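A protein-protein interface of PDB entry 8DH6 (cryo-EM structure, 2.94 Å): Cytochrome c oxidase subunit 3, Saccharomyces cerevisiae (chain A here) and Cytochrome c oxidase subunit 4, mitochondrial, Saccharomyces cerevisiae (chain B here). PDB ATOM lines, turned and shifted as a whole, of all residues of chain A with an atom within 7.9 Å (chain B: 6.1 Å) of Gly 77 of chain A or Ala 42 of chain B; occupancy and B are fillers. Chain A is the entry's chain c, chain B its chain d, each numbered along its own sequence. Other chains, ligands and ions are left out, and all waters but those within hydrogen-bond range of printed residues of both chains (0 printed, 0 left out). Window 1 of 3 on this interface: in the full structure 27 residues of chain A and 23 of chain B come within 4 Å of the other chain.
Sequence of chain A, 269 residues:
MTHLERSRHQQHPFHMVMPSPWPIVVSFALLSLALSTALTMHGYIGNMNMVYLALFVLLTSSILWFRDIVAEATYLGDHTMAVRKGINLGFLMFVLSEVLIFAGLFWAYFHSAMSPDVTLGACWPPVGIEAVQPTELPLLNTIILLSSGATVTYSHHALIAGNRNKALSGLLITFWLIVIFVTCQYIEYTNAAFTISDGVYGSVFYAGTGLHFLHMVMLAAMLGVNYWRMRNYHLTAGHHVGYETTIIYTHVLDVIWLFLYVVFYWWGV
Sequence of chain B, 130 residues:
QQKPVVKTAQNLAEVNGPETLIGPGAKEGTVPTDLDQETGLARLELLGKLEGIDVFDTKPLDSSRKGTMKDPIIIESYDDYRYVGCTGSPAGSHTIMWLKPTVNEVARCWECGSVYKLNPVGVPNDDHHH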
ATOM      1  N   PRO A  13     -21.891  28.848  34.644  1.00  0.00           N
ATOM      2  CA  PRO A  13     -21.619  27.819  33.627  1.00  0.00           C
ATOM      3  C   PRO A  13     -21.898  26.403  34.089  1.00  0.00           C
ATOM      4  O   PRO A  13     -22.002  25.504  33.245  1.00  0.00           O
ATOM      5  CB  PRO A  13     -20.124  28.007  33.322  1.00  0.00           C
ATOM      6  CG  PRO A  13     -19.732  29.300  33.969  1.00  0.00           C
ATOM      7  CD  PRO A  13     -20.659  29.495  35.115  1.00  0.00           C
ATOM      8  N   HIS A  15     -23.219  22.774  35.608  1.00  0.00           N
ATOM      9  CA  HIS A  15     -24.284  21.917  35.096  1.00  0.00           C
ATOM     10  C   HIS A  15     -25.129  21.386  36.247  1.00  0.00           C
ATOM     11  O   HIS A  15     -24.606  20.760  37.176  1.00  0.00           O
ATOM     12  CB  HIS A  15     -23.678  20.786  34.270  1.00  0.00           C
ATOM     13  CG  HIS A  15     -24.650  19.712  33.902  1.00  0.00           C
ATOM     14  ND1 HIS A  15     -25.811  19.963  33.206  1.00  0.00           N
ATOM     15  CD2 HIS A  15     -24.610  18.373  34.093  1.00  0.00           C
ATOM     16  CE1 HIS A  15     -26.460  18.830  33.010  1.00  0.00           C
ATOM     17  NE2 HIS A  15     -25.751  17.849  33.537  1.00  0.00           N
ATOM     18  N   VAL A  70     -23.850  11.441  27.658  1.00  0.00           N
ATOM     19  CA  VAL A  70     -23.701  11.900  26.280  1.00  0.00           C
ATOM     20  C   VAL A  70     -24.954  12.609  25.781  1.00  0.00           C
ATOM     21  O   VAL A  70     -24.844  13.511  24.941  1.00  0.00           O
ATOM     22  CB  VAL A  70     -23.325  10.756  25.320  1.00  0.00           C
ATOM     23  CG1 VAL A  70     -22.079  10.038  25.808  1.00  0.00           C
ATOM     24  CG2 VAL A  70     -24.472   9.785  25.141  1.00  0.00           C
ATOM     25  N   ALA A  71     -26.141  12.240  26.272  1.00  0.00           N
ATOM     26  CA  ALA A  71     -27.339  12.999  25.932  1.00  0.00           C
ATOM     27  C   ALA A  71     -27.248  14.421  26.464  1.00  0.00           C
ATOM     28  O   ALA A  71     -27.599  15.379  25.767  1.00  0.00           O
ATOM     29  CB  ALA A  71     -28.580  12.297  26.477  1.00  0.00           C
ATOM     30  N   GLU A  72     -26.777  14.579  27.703  1.00  0.00           N
ATOM     31  CA  GLU A  72     -26.598  15.921  28.250  1.00  0.00           C
ATOM     32  C   GLU A  72     -25.543  16.709  27.488  1.00  0.00           C
ATOM     33  O   GLU A  72     -25.748  17.891  27.196  1.00  0.00           O
ATOM     34  CB  GLU A  72     -26.218  15.857  29.727  1.00  0.00           C
ATOM     35  CG  GLU A  72     -27.202  15.114  30.594  1.00  0.00           C
ATOM     36  CD  GLU A  72     -26.668  14.875  31.986  1.00  0.00           C
ATOM     37  OE1 GLU A  72     -27.376  14.245  32.798  1.00  0.00           O
ATOM     38  OE2 GLU A  72     -25.537  15.317  32.269  1.00  0.00           O
ATOM     39  N   ALA A  73     -24.413  16.081  27.163  1.00  0.00           N
ATOM     40  CA  ALA A  73     -23.331  16.804  26.503  1.00  0.00           C
ATOM     41  C   ALA A  73     -23.702  17.201  25.079  1.00  0.00           C
ATOM     42  O   ALA A  73     -23.455  18.337  24.663  1.00  0.00           O
ATOM     43  CB  ALA A  73     -22.058  15.960  26.505  1.00  0.00           C
ATOM     44  N   THR A  74     -24.298  16.283  24.321  1.00  0.00           N
ATOM     45  CA  THR A  74     -24.559  16.510  22.906  1.00  0.00           C
ATOM     46  C   THR A  74     -25.926  17.131  22.653  1.00  0.00           C
ATOM     47  O   THR A  74     -26.038  18.108  21.908  1.00  0.00           O
ATOM     48  CB  THR A  74     -24.442  15.194  22.132  1.00  0.00           C
ATOM     49  OG1 THR A  74     -23.178  14.581  22.409  1.00  0.00           O
ATOM     50  CG2 THR A  74     -24.562  15.442  20.639  1.00  0.00           C
ATOM     51  N   TYR A  75     -26.993  16.587  23.207  1.00  0.00           N
ATOM     52  CA  TYR A  75     -28.338  17.053  22.804  1.00  0.00           C
ATOM     53  C   TYR A  75     -28.951  18.097  23.706  1.00  0.00           C
ATOM     54  O   TYR A  75     -29.868  18.719  23.268  1.00  0.00           O
ATOM     55  CB  TYR A  75     -29.256  15.859  22.794  1.00  0.00           C
ATOM     56  CG  TYR A  75     -28.858  14.721  21.904  1.00  0.00           C
ATOM     57  CD1 TYR A  75     -28.552  14.953  20.583  1.00  0.00           C
ATOM     58  CD2 TYR A  75     -28.832  13.421  22.372  1.00  0.00           C
ATOM     59  CE1 TYR A  75     -28.200  13.917  19.749  1.00  0.00           C
ATOM     60  CE2 TYR A  75     -28.479  12.371  21.548  1.00  0.00           C
ATOM     61  CZ  TYR A  75     -28.167  12.626  20.229  1.00  0.00           C
ATOM     62  OH  TYR A  75     -27.819  11.628  19.376  1.00  0.00           O
ATOM     63  N   LEU A  76     -28.513  18.225  24.940  1.00  0.00           N
ATOM     64  CA  LEU A  76     -28.974  19.333  25.765  1.00  0.00           C
ATOM     65  C   LEU A  76     -27.992  20.493  25.808  1.00  0.00           C
ATOM     66  O   LEU A  76     -28.378  21.594  26.212  1.00  0.00           O
ATOM     67  CB  LEU A  76     -29.261  18.850  27.190  1.00  0.00           C
ATOM     68  CG  LEU A  76     -30.611  18.182  27.456  1.00  0.00           C
ATOM     69  CD1 LEU A  76     -30.685  16.809  26.825  1.00  0.00           C
ATOM     70  CD2 LEU A  76     -30.862  18.089  28.945  1.00  0.00           C
ATOM     71  N   GLY A  77     -26.743  20.276  25.403  1.00  0.00           N
ATOM     72  CA  GLY A  77     -25.754  21.335  25.398  1.00  0.00           C
ATOM     73  C   GLY A  77     -25.428  21.907  26.754  1.00  0.00           C
ATOM     74  O   GLY A  77     -25.194  23.111  26.869  1.00  0.00           O
ATOM     75  N   ASP A  78     -25.408  21.075  27.791  1.00  0.00           N
ATOM     76  CA  ASP A  78     -25.141  21.551  29.141  1.00  0.00           C
ATOM     77  C   ASP A  78     -23.656  21.654  29.453  1.00  0.00           C
ATOM     78  O   ASP A  78     -23.295  22.218  30.491  1.00  0.00           O
ATOM     79  CB  ASP A  78     -25.812  20.631  30.156  1.00  0.00           C
ATOM     80  CG  ASP A  78     -27.311  20.821  30.211  1.00  0.00           C
ATOM     81  OD1 ASP A  78     -27.763  21.984  30.180  1.00  0.00           O
ATOM     82  OD2 ASP A  78     -28.041  19.811  30.285  1.00  0.00           O
ATOM     83  N   HIS A  79     -22.793  21.127  28.591  1.00  0.00           N
ATOM     84  CA  HIS A  79     -21.354  21.098  28.851  1.00  0.00           C
ATOM     85  C   HIS A  79     -20.728  22.385  28.332  1.00  0.00           C
ATOM     86  O   HIS A  79     -20.373  22.505  27.160  1.00  0.00           O
ATOM     87  CB  HIS A  79     -20.720  19.872  28.208  1.00  0.00           C
ATOM     88  CG  HIS A  79     -21.016  18.595  28.929  1.00  0.00           C
ATOM     89  ND1 HIS A  79     -20.066  17.619  29.135  1.00  0.00           N
ATOM     90  CD2 HIS A  79     -22.154  18.140  29.502  1.00  0.00           C
ATOM     91  CE1 HIS A  79     -20.610  16.613  29.796  1.00  0.00           C
ATOM     92  NE2 HIS A  79     -21.875  16.905  30.033  1.00  0.00           N
ATOM     93  N   THR A  80     -20.592  23.363  29.220  1.00  0.00           N
ATOM     94  CA  THR A  80     -19.901  24.602  28.900  1.00  0.00           C
ATOM     95  C   THR A  80     -18.408  24.412  29.171  1.00  0.00           C
ATOM     96  O   THR A  80     -17.951  23.292  29.417  1.00  0.00           O
ATOM     97  CB  THR A  80     -20.511  25.760  29.693  1.00  0.00           C
ATOM     98  OG1 THR A  80     -20.040  25.715  31.044  1.00  0.00           O
ATOM     99  CG2 THR A  80     -22.025  25.669  29.688  1.00  0.00           C
ATOM    100  N   MET A  81     -17.630  25.495  29.128  1.00  0.00           N
ATOM    101  CA  MET A  81     -16.185  25.376  29.291  1.00  0.00           C
ATOM    102  C   MET A  81     -15.816  24.881  30.686  1.00  0.00           C
ATOM    103  O   MET A  81     -14.933  24.025  30.834  1.00  0.00           O
ATOM    104  CB  MET A  81     -15.518  26.718  29.003  1.00  0.00           C
ATOM    105  CG  MET A  81     -15.360  27.034  27.524  1.00  0.00           C
ATOM    106  SD  MET A  81     -14.217  25.940  26.661  1.00  0.00           S
ATOM    107  CE  MET A  81     -12.857  25.855  27.825  1.00  0.00           C
ATOM    108  N   VAL A  83     -17.601  23.059  32.806  1.00  0.00           N
ATOM    109  CA  VAL A  83     -17.948  21.650  32.954  1.00  0.00           C
ATOM    110  C   VAL A  83     -16.928  20.767  32.246  1.00  0.00           C
ATOM    111  O   VAL A  83     -16.529  19.721  32.774  1.00  0.00           O
ATOM    112  CB  VAL A  83     -19.372  21.398  32.431  1.00  0.00           C
ATOM    113  CG1 VAL A  83     -19.828  20.002  32.796  1.00  0.00           C
ATOM    114  CG2 VAL A  83     -20.329  22.436  32.986  1.00  0.00           C
ATOM    115  N   ARG A  84     -16.495  21.167  31.049  1.00  0.00           N
ATOM    116  CA  ARG A  84     -15.495  20.395  30.320  1.00  0.00           C
ATOM    117  C   ARG A  84     -14.181  20.330  31.087  1.00  0.00           C
ATOM    118  O   ARG A  84     -13.565  19.260  31.191  1.00  0.00           O
ATOM    119  CB  ARG A  84     -15.282  21.007  28.937  1.00  0.00           C
ATOM    120  CG  ARG A  84     -16.468  20.838  28.013  1.00  0.00           C
ATOM    121  CD  ARG A  84     -16.084  20.989  26.555  1.00  0.00           C
ATOM    122  NE  ARG A  84     -16.065  22.375  26.105  1.00  0.00           N
ATOM    123  CZ  ARG A  84     -15.130  22.890  25.320  1.00  0.00           C
ATOM    124  NH1 ARG A  84     -14.116  22.163  24.883  1.00  0.00           N
ATOM    125  NH2 ARG A  84     -15.220  24.167  24.956  1.00  0.00           N
ATOM    126  N   HIS A 239     -15.296  20.787  20.227  1.00  0.00           N
ATOM    127  CA  HIS A 239     -15.929  20.365  21.476  1.00  0.00           C
ATOM    128  C   HIS A 239     -15.964  18.841  21.515  1.00  0.00           C
ATOM    129  O   HIS A 239     -16.875  18.213  20.970  1.00  0.00           O
ATOM    130  CB  HIS A 239     -17.328  20.960  21.606  1.00  0.00           C
ATOM    131  CG  HIS A 239     -18.101  20.438  22.776  1.00  0.00           C
ATOM    132  ND1 HIS A 239     -18.130  21.080  23.994  1.00  0.00           N
ATOM    133  CD2 HIS A 239     -18.881  19.340  22.912  1.00  0.00           C
ATOM    134  CE1 HIS A 239     -18.891  20.397  24.831  1.00  0.00           C
ATOM    135  NE2 HIS A 239     -19.357  19.335  24.200  1.00  0.00           N
ATOM    136  N   GLU B  38     -23.730  23.129  18.471  1.00  0.00           N
ATOM    137  CA  GLU B  38     -23.804  23.513  19.873  1.00  0.00           C
ATOM    138  C   GLU B  38     -25.200  24.033  20.190  1.00  0.00           C
ATOM    139  O   GLU B  38     -25.823  24.719  19.376  1.00  0.00           O
ATOM    140  CB  GLU B  38     -22.760  24.576  20.207  1.00  0.00           C
ATOM    141  CG  GLU B  38     -21.371  24.025  20.477  1.00  0.00           C
ATOM    142  CD  GLU B  38     -21.369  22.913  21.506  1.00  0.00           C
ATOM    143  OE1 GLU B  38     -22.035  23.062  22.552  1.00  0.00           O
ATOM    144  OE2 GLU B  38     -20.699  21.886  21.269  1.00  0.00           O
ATOM    145  N   THR B  39     -25.698  23.698  21.377  1.00  0.00           N
ATOM    146  CA  THR B  39     -27.054  24.047  21.764  1.00  0.00           C
ATOM    147  C   THR B  39     -27.097  24.464  23.227  1.00  0.00           C
ATOM    148  O   THR B  39     -26.213  24.136  24.021  1.00  0.00           O
ATOM    149  CB  THR B  39     -28.021  22.884  21.513  1.00  0.00           C
ATOM    150  OG1 THR B  39     -29.359  23.305  21.795  1.00  0.00           O
ATOM    151  CG2 THR B  39     -27.670  21.705  22.391  1.00  0.00           C
ATOM    152  N   GLY B  40     -28.141  25.216  23.569  1.00  0.00           N
ATOM    153  CA  GLY B  40     -28.391  25.558  24.959  1.00  0.00           C
ATOM    154  C   GLY B  40     -27.347  26.492  25.540  1.00  0.00           C
ATOM    155  O   GLY B  40     -26.869  27.427  24.888  1.00  0.00           O
ATOM    156  N   LEU B  41     -26.998  26.234  26.803  1.00  0.00           N
ATOM    157  CA  LEU B  41     -26.085  27.110  27.528  1.00  0.00           C
ATOM    158  C   LEU B  41     -24.704  27.154  26.890  1.00  0.00           C
ATOM    159  O   LEU B  41     -24.073  28.218  26.857  1.00  0.00           O
ATOM    160  CB  LEU B  41     -25.980  26.657  28.981  1.00  0.00           C
ATOM    161  CG  LEU B  41     -25.620  27.739  29.994  1.00  0.00           C
ATOM    162  CD1 LEU B  41     -26.728  28.770  30.092  1.00  0.00           C
ATOM    163  CD2 LEU B  41     -25.329  27.121  31.344  1.00  0.00           C
ATOM    164  N   ALA B  42     -24.211  26.018  26.396  1.00  0.00           N
ATOM    165  CA  ALA B  42     -22.920  26.013  25.718  1.00  0.00           C
ATOM    166  C   ALA B  42     -22.957  26.865  24.456  1.00  0.00           C
ATOM    167  O   ALA B  42     -22.004  27.595  24.167  1.00  0.00           O
ATOM    168  CB  ALA B  42     -22.504  24.582  25.393  1.00  0.00           C
ATOM    169  N   ARG B  43     -24.052  26.789  23.695  1.00  0.00           N
ATOM    170  CA  ARG B  43     -24.198  27.635  22.514  1.00  0.00           C
ATOM    171  C   ARG B  43     -24.247  29.108  22.892  1.00  0.00           C
ATOM    172  O   ARG B  43     -23.662  29.953  22.206  1.00  0.00           O
ATOM    173  CB  ARG B  43     -25.456  27.242  21.745  1.00  0.00           C
ATOM    174  CG  ARG B  43     -25.734  28.085  20.519  1.00  0.00           C
ATOM    175  CD  ARG B  43     -24.681  27.869  19.458  1.00  0.00           C
ATOM    176  NE  ARG B  43     -25.111  28.371  18.160  1.00  0.00           N
ATOM    177  CZ  ARG B  43     -25.786  27.661  17.269  1.00  0.00           C
ATOM    178  NH1 ARG B  43     -26.137  26.409  17.507  1.00  0.00           N
ATOM    179  NH2 ARG B  43     -26.118  28.220  16.110  1.00  0.00           N
ATOM    180  N   LEU B  44     -24.955  29.438  23.974  1.00  0.00           N
ATOM    181  CA  LEU B  44     -25.025  30.827  24.419  1.00  0.00           C
ATOM    182  C   LEU B  44     -23.649  31.347  24.823  1.00  0.00           C
ATOM    183  O   LEU B  44     -23.263  32.466  24.456  1.00  0.00           O
ATOM    184  CB  LEU B  44     -26.006  30.947  25.584  1.00  0.00           C
ATOM    185  CG  LEU B  44     -26.267  32.353  26.113  1.00  0.00           C
ATOM    186  CD1 LEU B  44     -27.205  33.067  25.170  1.00  0.00           C
ATOM    187  CD2 LEU B  44     -26.843  32.314  27.518  1.00  0.00           C
ATOM    188  N   GLU B  45     -22.894  30.539  25.570  1.00  0.00           N
ATOM    189  CA  GLU B  45     -21.540  30.922  25.955  1.00  0.00           C
ATOM    190  C   GLU B  45     -20.641  31.078  24.734  1.00  0.00           C
ATOM    191  O   GLU B  45     -19.838  32.016  24.662  1.00  0.00           O
ATOM    192  CB  GLU B  45     -20.967  29.889  26.926  1.00  0.00           C
ATOM    193  CG  GLU B  45     -19.455  29.785  26.921  1.00  0.00           C
ATOM    194  CD  GLU B  45     -18.796  30.835  27.789  1.00  0.00           C
ATOM    195  OE1 GLU B  45     -19.514  31.514  28.551  1.00  0.00           O
ATOM    196  OE2 GLU B  45     -17.559  30.985  27.706  1.00  0.00           O
ATOM    197  N   LEU B  46     -20.767  30.171  23.762  1.00  0.00           N
ATOM    198  CA  LEU B  46     -19.984  30.280  22.535  1.00  0.00           C
ATOM    199  C   LEU B  46     -20.300  31.571  21.792  1.00  0.00           C
ATOM    200  O   LEU B  46     -19.386  32.269  21.337  1.00  0.00           O
ATOM    201  CB  LEU B  46     -20.249  29.073  21.639  1.00  0.00           C
ATOM    202  CG  LEU B  46     -19.565  29.076  20.275  1.00  0.00           C
ATOM    203  CD1 LEU B  46     -18.081  28.774  20.419  1.00  0.00           C
ATOM    204  CD2 LEU B  46     -20.238  28.096  19.335  1.00  0.00           C
ATOM    205  N   LEU B  47     -21.585  31.908  21.665  1.00  0.00           N
ATOM    206  CA  LEU B  47     -21.955  33.177  21.050  1.00  0.00           C
ATOM    207  C   LEU B  47     -21.302  34.340  21.782  1.00  0.00           C
ATOM    208  O   LEU B  47     -20.610  35.161  21.166  1.00  0.00           O
ATOM    209  CB  LEU B  47     -23.474  33.335  21.040  1.00  0.00           C
ATOM    210  CG  LEU B  47     -24.263  32.453  20.073  1.00  0.00           C
ATOM    211  CD1 LEU B  47     -25.735  32.809  20.125  1.00  0.00           C
ATOM    212  CD2 LEU B  47     -23.727  32.597  18.662  1.00  0.00           C
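Of the 17 printed residues of chain A, 7 touch a printed residue of chain B.
Printed residues of chain B that touch a printed residue of chain A: Glu 38, Thr 39, Leu 41 and Ala 42.
Along chain B the printed residues that touch a printed residue of chain A span positions 38 to 42.
Among the printed residues, no Asp or Glu carboxylate lies within 4 Å of a Lys or Arg side-chain nitrogen of the other chain.
O of Pro 13 of chain A sits at hydrogen-bond distance from OG1 of Thr 80 of chain A.
OG1 of Thr 74 of chain A is in hydrogen-bond range of O of Val 70 of chain A.
The backbone NH (N) of Leu 76 of chain A is in hydrogen-bond range of the backbone carbonyl oxygen (O) of Ala 71 of chain A (3.1 Å).
O of Glu 72 of chain A lies within hydrogen-bond range of N of Gly 77 of chain A (3.1 Å).
ND1 of His 239 of chain A is in hydrogen-bond range of NE of Arg 84 of chain A (3.2 Å).
The backbone carbonyl oxygen (O) of Glu 38 of chain B sits at hydrogen-bond distance from the guanidinium group (NH1) of Arg 43 of chain B (2.5 Å).
Thr 39 of chain B touches Thr 74 of chain A.
O of Tyr 75 of chain A touches CG2 of Thr 39 of chain B, 3.8 Å away.
Leu 76 of chain A touches Thr 39 of chain B (C to CG2, 3.6 Å).
Gly 77 of chain A touches Leu 41 of chain B.
His 79 of chain A touches Ala 42 of chain B (O to CB, 3.5 Å).
Leu 41 of chain B touches Thr 80 of chain A.
N of Ala 42 of chain B touches CG2 of Thr 80 of chain A, 3.97 Å away.
CG of His 239 of chain A touches OE2 of Glu 38 of chain B, at 3.3 Å.
O of Gly 77 of chain A is in hydrogen-bond range of N of Ala 42 of chain B, 3.1 Å away.
O of Gly 77 of chain A sits close to O of Thr 39 of chain B, 3.2 Å away.
Of the printed residues of chain B, Leu 76 of chain A touches Thr 39 (3.6 Å).
Gly 77 of chain A touches just these residues of chain B: Thr 39 (3.2 Å), Leu 41 (3.6 Å) and Ala 42 (3.1 Å).
Of the printed residues of chain B, His 79 of chain A touches Ala 42.
Printed residues of chain B within 4 Å of His 239 of chain A: Glu 38.
Of the printed residues of chain A, Thr 39 of chain B touches Thr 74 (3.98 Å), Tyr 75 (3.8 Å), Leu 76 (3.6 Å) and Gly 77 (3.2 Å).
Of the printed residues of chain A, Leu 41 of chain B touches Gly 77 and Thr 80.
Of chain A, only Gly 77 (3.1 Å), His 79 (3.5 Å) and Thr 80 (3.97 Å) come within 4 Å of Ala 42 of chain B.
The nearest residue of chain B that does not touch Gly 77 of chain A is Gly 40 of chain B (4.2 Å).
The nearest residue of chain A that does not touch Ala 42 of chain B is Asp 78 of chain A (5.1 Å).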
